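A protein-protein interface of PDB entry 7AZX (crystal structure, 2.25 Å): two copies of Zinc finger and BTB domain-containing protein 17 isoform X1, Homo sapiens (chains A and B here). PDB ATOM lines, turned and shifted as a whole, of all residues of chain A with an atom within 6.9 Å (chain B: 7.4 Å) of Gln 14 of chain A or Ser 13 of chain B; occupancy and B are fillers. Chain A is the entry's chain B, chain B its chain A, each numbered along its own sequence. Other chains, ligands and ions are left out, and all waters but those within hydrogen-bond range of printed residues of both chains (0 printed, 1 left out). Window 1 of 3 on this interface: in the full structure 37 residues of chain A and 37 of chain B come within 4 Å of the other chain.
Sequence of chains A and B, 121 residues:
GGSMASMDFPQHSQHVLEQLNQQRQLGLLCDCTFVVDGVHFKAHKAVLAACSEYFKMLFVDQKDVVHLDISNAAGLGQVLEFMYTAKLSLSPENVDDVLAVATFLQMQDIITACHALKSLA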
ATOM      1  N   PHE A   9      23.348   6.970  31.378  1.00  0.00           N
ATOM      2  CA  PHE A   9      23.307   6.599  29.963  1.00  0.00           C
ATOM      3  C   PHE A   9      23.202   5.084  29.852  1.00  0.00           C
ATOM      4  O   PHE A   9      24.219   4.377  29.958  1.00  0.00           O
ATOM      5  CB  PHE A   9      24.546   7.110  29.228  1.00  0.00           C
ATOM      6  CG  PHE A   9      24.521   8.587  28.957  1.00  0.00           C
ATOM      7  CD1 PHE A   9      24.774   9.497  29.972  1.00  0.00           C
ATOM      8  CD2 PHE A   9      24.245   9.068  27.687  1.00  0.00           C
ATOM      9  CE1 PHE A   9      24.753  10.857  29.727  1.00  0.00           C
ATOM     10  CE2 PHE A   9      24.222  10.428  27.435  1.00  0.00           C
ATOM     11  CZ  PHE A   9      24.476  11.323  28.457  1.00  0.00           C
ATOM     12  N   PRO A  10      21.998   4.540  29.643  1.00  0.00           N
ATOM     13  CA  PRO A  10      21.849   3.076  29.640  1.00  0.00           C
ATOM     14  C   PRO A  10      22.568   2.389  28.493  1.00  0.00           C
ATOM     15  O   PRO A  10      22.947   1.219  28.632  1.00  0.00           O
ATOM     16  CB  PRO A  10      20.329   2.877  29.548  1.00  0.00           C
ATOM     17  CG  PRO A  10      19.733   4.189  29.970  1.00  0.00           C
ATOM     18  CD  PRO A  10      20.705   5.230  29.515  1.00  0.00           C
ATOM     19  N   GLN A  11      22.775   3.071  27.367  1.00  0.00           N
ATOM     20  CA  GLN A  11      23.417   2.473  26.205  1.00  0.00           C
ATOM     21  C   GLN A  11      24.910   2.776  26.141  1.00  0.00           C
ATOM     22  O   GLN A  11      25.525   2.618  25.082  1.00  0.00           O
ATOM     23  CB  GLN A  11      22.724   2.937  24.923  1.00  0.00           C
ATOM     24  CG  GLN A  11      21.200   2.894  24.985  1.00  0.00           C
ATOM     25  CD  GLN A  11      20.632   1.495  24.794  1.00  0.00           C
ATOM     26  OE1 GLN A  11      21.007   0.555  25.496  1.00  0.00           O
ATOM     27  NE2 GLN A  11      19.717   1.357  23.843  1.00  0.00           N
ATOM     28  N   HIS A  12      25.508   3.196  27.257  1.00  0.00           N
ATOM     29  CA  HIS A  12      26.931   3.519  27.250  1.00  0.00           C
ATOM     30  C   HIS A  12      27.792   2.261  27.297  1.00  0.00           C
ATOM     31  O   HIS A  12      28.704   2.096  26.479  1.00  0.00           O
ATOM     32  CB  HIS A  12      27.271   4.440  28.422  1.00  0.00           C
ATOM     33  CG  HIS A  12      28.734   4.727  28.557  1.00  0.00           C
ATOM     34  ND1 HIS A  12      29.419   5.526  27.668  1.00  0.00           N
ATOM     35  CD2 HIS A  12      29.642   4.319  29.475  1.00  0.00           C
ATOM     36  CE1 HIS A  12      30.687   5.600  28.033  1.00  0.00           C
ATOM     37  NE2 HIS A  12      30.849   4.877  29.126  1.00  0.00           N
ATOM     38  N   SER A  13      27.514   1.366  28.249  1.00  0.00           N
ATOM     39  CA  SER A  13      28.319   0.156  28.391  1.00  0.00           C
ATOM     40  C   SER A  13      28.250  -0.707  27.138  1.00  0.00           C
ATOM     41  O   SER A  13      29.233  -1.360  26.770  1.00  0.00           O
ATOM     42  CB  SER A  13      27.855  -0.634  29.612  1.00  0.00           C
ATOM     43  OG  SER A  13      26.670  -1.347  29.325  1.00  0.00           O
ATOM     44  N   GLN A  14      27.092  -0.736  26.478  1.00  0.00           N
ATOM     45  CA  GLN A  14      26.993  -1.428  25.198  1.00  0.00           C
ATOM     46  C   GLN A  14      27.826  -0.725  24.133  1.00  0.00           C
ATOM     47  O   GLN A  14      28.434  -1.380  23.279  1.00  0.00           O
ATOM     48  CB  GLN A  14      25.529  -1.523  24.764  1.00  0.00           C
ATOM     49  CG  GLN A  14      25.313  -2.274  23.462  1.00  0.00           C
ATOM     50  CD  GLN A  14      23.863  -2.270  23.012  1.00  0.00           C
ATOM     51  OE1 GLN A  14      23.040  -1.508  23.521  1.00  0.00           O
ATOM     52  NE2 GLN A  14      23.546  -3.127  22.049  1.00  0.00           N
ATOM     53  N   HIS A  15      27.872   0.608  24.174  1.00  0.00           N
ATOM     54  CA  HIS A  15      28.665   1.351  23.201  1.00  0.00           C
ATOM     55  C   HIS A  15      30.157   1.160  23.442  1.00  0.00           C
ATOM     56  O   HIS A  15      30.940   1.074  22.488  1.00  0.00           O
ATOM     57  CB  HIS A  15      28.296   2.834  23.249  1.00  0.00           C
ATOM     58  CG  HIS A  15      29.140   3.696  22.362  1.00  0.00           C
ATOM     59  ND1 HIS A  15      30.235   4.394  22.826  1.00  0.00           N
ATOM     60  CD2 HIS A  15      29.052   3.972  21.038  1.00  0.00           C
ATOM     61  CE1 HIS A  15      30.783   5.062  21.828  1.00  0.00           C
ATOM     62  NE2 HIS A  15      30.085   4.824  20.732  1.00  0.00           N
ATOM     63  N   VAL A  16      30.570   1.091  24.710  1.00  0.00           N
ATOM     64  CA  VAL A  16      31.981   0.885  25.021  1.00  0.00           C
ATOM     65  C   VAL A  16      32.430  -0.499  24.570  1.00  0.00           C
ATOM     66  O   VAL A  16      33.517  -0.659  23.999  1.00  0.00           O
ATOM     67  CB  VAL A  16      32.237   1.101  26.523  1.00  0.00           C
ATOM     68  CG1 VAL A  16      33.698   0.843  26.858  1.00  0.00           C
ATOM     69  CG2 VAL A  16      31.845   2.509  26.929  1.00  0.00           C
ATOM     70  N   LEU A  17      31.605  -1.520  24.813  1.00  0.00           N
ATOM     71  CA  LEU A  17      31.973  -2.876  24.419  1.00  0.00           C
ATOM     72  C   LEU A  17      32.053  -3.011  22.903  1.00  0.00           C
ATOM     73  O   LEU A  17      32.934  -3.704  22.382  1.00  0.00           O
ATOM     74  CB  LEU A  17      30.976  -3.880  24.997  1.00  0.00           C
ATOM     75  CG  LEU A  17      31.337  -5.358  24.833  1.00  0.00           C
ATOM     76  CD1 LEU A  17      32.659  -5.666  25.517  1.00  0.00           C
ATOM     77  CD2 LEU A  17      30.229  -6.250  25.374  1.00  0.00           C
ATOM     78  N   GLU A  18      31.142  -2.354  22.178  1.00  0.00           N
ATOM     79  CA  GLU A  18      31.194  -2.393  20.721  1.00  0.00           C
ATOM     80  C   GLU A  18      32.444  -1.701  20.194  1.00  0.00           C
ATOM     81  O   GLU A  18      33.071  -2.180  19.241  1.00  0.00           O
ATOM     82  CB  GLU A  18      29.937  -1.755  20.130  1.00  0.00           C
ATOM     83  CG  GLU A  18      28.691  -2.618  20.245  1.00  0.00           C
ATOM     84  CD  GLU A  18      27.434  -1.893  19.804  1.00  0.00           C
ATOM     85  OE1 GLU A  18      26.326  -2.377  20.115  1.00  0.00           O
ATOM     86  OE2 GLU A  18      27.553  -0.838  19.143  1.00  0.00           O
ATOM     87  N   GLN A  19      32.826  -0.575  20.803  1.00  0.00           N
ATOM     88  CA  GLN A  19      34.049   0.105  20.389  1.00  0.00           C
ATOM     89  C   GLN A  19      35.280  -0.724  20.729  1.00  0.00           C
ATOM     90  O   GLN A  19      36.237  -0.772  19.947  1.00  0.00           O
ATOM     91  CB  GLN A  19      34.129   1.486  21.039  1.00  0.00           C
ATOM     92  CG  GLN A  19      33.223   2.520  20.394  1.00  0.00           C
ATOM     93  CD  GLN A  19      33.583   2.783  18.945  1.00  0.00           C
ATOM     94  OE1 GLN A  19      34.748   2.997  18.613  1.00  0.00           O
ATOM     95  NE2 GLN A  19      32.581   2.763  18.074  1.00  0.00           N
ATOM     96  N   TYR A  84      33.545  -9.719  23.605  1.00  0.00           N
ATOM     97  CA  TYR A  84      33.448  -8.407  22.984  1.00  0.00           C
ATOM     98  C   TYR A  84      32.070  -8.100  22.410  1.00  0.00           C
ATOM     99  O   TYR A  84      31.811  -6.944  22.060  1.00  0.00           O
ATOM    100  CB  TYR A  84      34.502  -8.273  21.877  1.00  0.00           C
ATOM    101  CG  TYR A  84      35.913  -8.085  22.393  1.00  0.00           C
ATOM    102  CD1 TYR A  84      36.418  -6.815  22.642  1.00  0.00           C
ATOM    103  CD2 TYR A  84      36.739  -9.177  22.629  1.00  0.00           C
ATOM    104  CE1 TYR A  84      37.706  -6.637  23.113  1.00  0.00           C
ATOM    105  CE2 TYR A  84      38.028  -9.009  23.102  1.00  0.00           C
ATOM    106  CZ  TYR A  84      38.506  -7.737  23.341  1.00  0.00           C
ATOM    107  OH  TYR A  84      39.788  -7.563  23.809  1.00  0.00           O
ATOM    108  N   ALA A  86      29.016  -9.996  23.780  1.00  0.00           N
ATOM    109  CA  ALA A  86      28.029 -10.516  24.724  1.00  0.00           C
ATOM    110  C   ALA A  86      27.106 -11.560  24.105  1.00  0.00           C
ATOM    111  O   ALA A  86      26.066 -11.885  24.692  1.00  0.00           O
ATOM    112  CB  ALA A  86      27.193  -9.390  25.346  1.00  0.00           C
ATOM    113  N   ASP B   8      22.291 -14.685  24.176  1.00  0.00           N
ATOM    114  CA  ASP B   8      22.679 -13.301  24.423  1.00  0.00           C
ATOM    115  C   ASP B   8      22.607 -13.018  25.916  1.00  0.00           C
ATOM    116  O   ASP B   8      21.611 -13.351  26.569  1.00  0.00           O
ATOM    117  CB  ASP B   8      21.772 -12.335  23.648  1.00  0.00           C
ATOM    118  CG  ASP B   8      22.080 -10.875  23.938  1.00  0.00           C
ATOM    119  OD1 ASP B   8      23.026 -10.325  23.334  1.00  0.00           O
ATOM    120  OD2 ASP B   8      21.367 -10.274  24.768  1.00  0.00           O
ATOM    121  N   PHE B   9      23.665 -12.412  26.454  1.00  0.00           N
ATOM    122  CA  PHE B   9      23.717 -12.036  27.866  1.00  0.00           C
ATOM    123  C   PHE B   9      23.598 -10.523  27.977  1.00  0.00           C
ATOM    124  O   PHE B   9      24.608  -9.811  27.847  1.00  0.00           O
ATOM    125  CB  PHE B   9      25.015 -12.525  28.515  1.00  0.00           C
ATOM    126  CG  PHE B   9      25.089 -14.018  28.679  1.00  0.00           C
ATOM    127  CD1 PHE B   9      25.352 -14.833  27.591  1.00  0.00           C
ATOM    128  CD2 PHE B   9      24.898 -14.606  29.919  1.00  0.00           C
ATOM    129  CE1 PHE B   9      25.423 -16.206  27.733  1.00  0.00           C
ATOM    130  CE2 PHE B   9      24.967 -15.983  30.069  1.00  0.00           C
ATOM    131  CZ  PHE B   9      25.230 -16.782  28.974  1.00  0.00           C
ATOM    132  N   PRO B  10      22.403  -9.981  28.214  1.00  0.00           N
ATOM    133  CA  PRO B  10      22.234  -8.520  28.174  1.00  0.00           C
ATOM    134  C   PRO B  10      23.005  -7.777  29.249  1.00  0.00           C
ATOM    135  O   PRO B  10      23.284  -6.584  29.073  1.00  0.00           O
ATOM    136  CB  PRO B  10      20.718  -8.334  28.349  1.00  0.00           C
ATOM    137  CG  PRO B  10      20.117  -9.670  28.023  1.00  0.00           C
ATOM    138  CD  PRO B  10      21.129 -10.678  28.460  1.00  0.00           C
ATOM    139  N   GLN B  11      23.362  -8.429  30.350  1.00  0.00           N
ATOM    140  CA  GLN B  11      24.080  -7.766  31.429  1.00  0.00           C
ATOM    141  C   GLN B  11      25.594  -7.899  31.307  1.00  0.00           C
ATOM    142  O   GLN B  11      26.313  -7.527  32.240  1.00  0.00           O
ATOM    143  CB  GLN B  11      23.614  -8.311  32.781  1.00  0.00           C
ATOM    144  CG  GLN B  11      22.563  -7.448  33.463  1.00  0.00           C
ATOM    145  CD  GLN B  11      22.912  -5.971  33.435  1.00  0.00           C
ATOM    146  OE1 GLN B  11      23.741  -5.506  34.218  1.00  0.00           O
ATOM    147  NE2 GLN B  11      22.276  -5.225  32.535  1.00  0.00           N
ATOM    148  N   HIS B  12      26.095  -8.410  30.178  1.00  0.00           N
ATOM    149  CA  HIS B  12      27.533  -8.621  30.037  1.00  0.00           C
ATOM    150  C   HIS B  12      28.276  -7.306  29.843  1.00  0.00           C
ATOM    151  O   HIS B  12      29.369  -7.121  30.391  1.00  0.00           O
ATOM    152  CB  HIS B  12      27.815  -9.569  28.872  1.00  0.00           C
ATOM    153  CG  HIS B  12      29.274  -9.757  28.587  1.00  0.00           C
ATOM    154  ND1 HIS B  12      30.073 -10.605  29.325  1.00  0.00           N
ATOM    155  CD2 HIS B  12      30.079  -9.206  27.647  1.00  0.00           C
ATOM    156  CE1 HIS B  12      31.305 -10.568  28.852  1.00  0.00           C
ATOM    157  NE2 HIS B  12      31.337  -9.728  27.834  1.00  0.00           N
ATOM    158  N   SER B  13      27.708  -6.383  29.062  1.00  0.00           N
ATOM    159  CA  SER B  13      28.379  -5.110  28.814  1.00  0.00           C
ATOM    160  C   SER B  13      28.559  -4.318  30.102  1.00  0.00           C
ATOM    161  O   SER B  13      29.628  -3.741  30.341  1.00  0.00           O
ATOM    162  CB  SER B  13      27.593  -4.293  27.789  1.00  0.00           C
ATOM    163  OG  SER B  13      26.487  -3.645  28.395  1.00  0.00           O
ATOM    164  N   GLN B  14      27.527  -4.280  30.948  1.00  0.00           N
ATOM    165  CA  GLN B  14      27.641  -3.564  32.213  1.00  0.00           C
ATOM    166  C   GLN B  14      28.602  -4.261  33.169  1.00  0.00           C
ATOM    167  O   GLN B  14      29.287  -3.593  33.951  1.00  0.00           O
ATOM    168  CB  GLN B  14      26.263  -3.412  32.859  1.00  0.00           C
ATOM    169  CG  GLN B  14      26.219  -2.416  34.010  1.00  0.00           C
ATOM    170  CD  GLN B  14      26.528  -0.997  33.569  1.00  0.00           C
ATOM    171  OE1 GLN B  14      25.738  -0.366  32.867  1.00  0.00           O
ATOM    172  NE2 GLN B  14      27.684  -0.488  33.983  1.00  0.00           N
ATOM    173  N   HIS B  15      28.673  -5.593  33.118  1.00  0.00           N
ATOM    174  CA  HIS B  15      29.567  -6.317  34.016  1.00  0.00           C
ATOM    175  C   HIS B  15      31.028  -6.088  33.648  1.00  0.00           C
ATOM    176  O   HIS B  15      31.876  -5.918  34.533  1.00  0.00           O
ATOM    177  CB  HIS B  15      29.234  -7.808  34.001  1.00  0.00           C
ATOM    178  CG  HIS B  15      28.027  -8.165  34.810  1.00  0.00           C
ATOM    179  ND1 HIS B  15      27.372  -9.370  34.681  1.00  0.00           N
ATOM    180  CD2 HIS B  15      27.354  -7.472  35.760  1.00  0.00           C
ATOM    181  CE1 HIS B  15      26.348  -9.406  35.516  1.00  0.00           C
ATOM    182  NE2 HIS B  15      26.316  -8.266  36.183  1.00  0.00           N
ATOM    183  N   VAL B  16      31.342  -6.081  32.351  1.00  0.00           N
ATOM    184  CA  VAL B  16      32.715  -5.827  31.923  1.00  0.00           C
ATOM    185  C   VAL B  16      33.121  -4.399  32.262  1.00  0.00           C
ATOM    186  O   VAL B  16      34.267  -4.139  32.652  1.00  0.00           O
ATOM    187  CB  VAL B  16      32.870  -6.121  30.419  1.00  0.00           C
ATOM    188  CG1 VAL B  16      34.278  -5.788  29.952  1.00  0.00           C
ATOM    189  CG2 VAL B  16      32.542  -7.574  30.129  1.00  0.00           C
ATOM    190  N   LEU B  17      32.190  -3.452  32.128  1.00  0.00           N
ATOM    191  CA  LEU B  17      32.499  -2.060  32.441  1.00  0.00           C
ATOM    192  C   LEU B  17      32.777  -1.874  33.928  1.00  0.00           C
ATOM    193  O   LEU B  17      33.659  -1.092  34.307  1.00  0.00           O
ATOM    194  CB  LEU B  17      31.354  -1.156  31.990  1.00  0.00           C
ATOM    195  CG  LEU B  17      31.666   0.341  31.927  1.00  0.00           C
ATOM    196  CD1 LEU B  17      32.721   0.619  30.868  1.00  0.00           C
ATOM    197  CD2 LEU B  17      30.402   1.140  31.655  1.00  0.00           C
ATOM    198  N   GLU B  18      32.035  -2.578  34.787  1.00  0.00           N
ATOM    199  CA  GLU B  18      32.299  -2.497  36.220  1.00  0.00           C
ATOM    200  C   GLU B  18      33.653  -3.099  36.575  1.00  0.00           C
ATOM    201  O   GLU B  18      34.331  -2.604  37.483  1.00  0.00           O
ATOM    202  CB  GLU B  18      31.183  -3.190  37.004  1.00  0.00           C
ATOM    203  CG  GLU B  18      29.833  -2.497  36.898  1.00  0.00           C
ATOM    204  CD  GLU B  18      28.693  -3.353  37.418  1.00  0.00           C
ATOM    205  OE1 GLU B  18      27.891  -2.849  38.234  1.00  0.00           O
ATOM    206  OE2 GLU B  18      28.600  -4.531  37.013  1.00  0.00           O
ATOM    207  N   GLN B  19      34.061  -4.160  35.876  1.00  0.00           N
ATOM    208  CA  GLN B  19      35.397  -4.706  36.086  1.00  0.00           C
ATOM    209  C   GLN B  19      36.465  -3.733  35.606  1.00  0.00           C
ATOM    210  O   GLN B  19      37.491  -3.549  36.271  1.00  0.00           O
ATOM    211  CB  GLN B  19      35.534  -6.051  35.375  1.00  0.00           C
ATOM    212  CG  GLN B  19      34.645  -7.149  35.936  1.00  0.00           C
ATOM    213  CD  GLN B  19      35.307  -7.921  37.062  1.00  0.00           C
ATOM    214  OE1 GLN B  19      36.293  -7.469  37.647  1.00  0.00           O
ATOM    215  NE2 GLN B  19      34.768  -9.096  37.369  1.00  0.00           N
ATOM    216  N   LEU B  20      36.240  -3.100  34.450  1.00  0.00           N
ATOM    217  CA  LEU B  20      37.167  -2.079  33.973  1.00  0.00           C
ATOM    218  C   LEU B  20      37.241  -0.901  34.934  1.00  0.00           C
ATOM    219  O   LEU B  20      38.299  -0.276  35.070  1.00  0.00           O
ATOM    220  CB  LEU B  20      36.752  -1.599  32.582  1.00  0.00           C
ATOM    221  CG  LEU B  20      36.890  -2.601  31.435  1.00  0.00           C
ATOM    222  CD1 LEU B  20      36.437  -1.976  30.125  1.00  0.00           C
ATOM    223  CD2 LEU B  20      38.322  -3.102  31.328  1.00  0.00           C
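The side-chain amide nitrogen (NE2) of Gln 14 of chain A sits at hydrogen-bond distance from the side-chain carboxylate (OE1) of Glu 18 of chain A.
Gln 11 of chain A touches none of the printed residues of chain B. Of the printed residues of chain B, His 12 of chain A touches Leu 17. Of chain B, only Ser 13 (3.5 Å) comes within 4 Å of Gln 14 of chain A. Printed residues of chain A within 4 Å of Asp 8 of chain B: Ala 86. Printed residues of chain A within 4 Å of His 12 of chain B: Leu 17 (3.7 Å) and Ala 86 (3.6 Å). Ser 13 of chain B touches just these residues of chain A: Ser 13 and Gln 14. Of the printed residues of chain A, Leu 17 of chain B touches His 12 (3.9 Å) and Ser 13 (3.7 Å). The nearest printed residue of chain B that does not touch Leu 17 of chain A is Ser 13 of chain B (4.1 Å).
Hydrophobic or aromatic side chains of chain B that line the printed part of chain A: His 12 and Leu 17. Of the 13 printed residues of chain A, 5 touch a printed residue of chain B. Printed residues of chain A that touch a printed residue of chain B: His 12, Ser 13, Gln 14, Leu 17 and Ala 86. Hydrophobic or aromatic side chains of chain A within 4 Å of the printed part of chain B: His 12, Leu 17 and Ala 86. Among the printed residues, no Asp or Glu carboxylate lies within 4 Å of a Lys or Arg side-chain nitrogen of the other chain.
Among the printed residues, merely in contact across the chains: Gln 14 of chain A with Ser 13 of chain B (3.5 Å), Ala 86 of chain A with His 12 of chain B (3.6 Å), Ala 86 of chain A with Asp 8 of chain B (3.7 Å), Ser 13 of chain A with Leu 17 of chain B (3.7 Å), Leu 17 of chain A with His 12 of chain B (3.7 Å) and His 12 of chain A with Leu 17 of chain B (3.9 Å).
His 12 of chain A touches Leu 17 of chain B, and with the chains exchanged Leu 17 of chain A touches His 12 of chain B. Ser 13 of chain A touches its own counterpart, Ser 13 of chain B. Ser 13 of chain A touches Gln 14 of chain B, and with the chains exchanged Gln 14 of chain A touches Ser 13 of chain B. Ser 13 of chain A touches Leu 17 of chain B, but with the chains exchanged Leu 17 of chain A does not touch Ser 13 of chain B (4.1 Å). 11 positions are printed for both chains. Of the 9 pairs that touch across the chains among the printed residues, 5 have their exchanged pair printed and touching as well.
The backbone NH (N) of Phe 9 of chain B sits at hydrogen-bond distance from the backbone carbonyl oxygen (O) of Ala 86 of chain A, 3.0 Å away. The side-chain hydroxyl of Ser 13 of chain A is in hydrogen-bond range of the side-chain hydroxyl of Ser 13 of chain B (2.5 Å). The side-chain hydroxyl of Ser 13 of chain A lies within hydrogen-bond range of the backbone NH of Gln 14 of chain B (3.5 Å).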
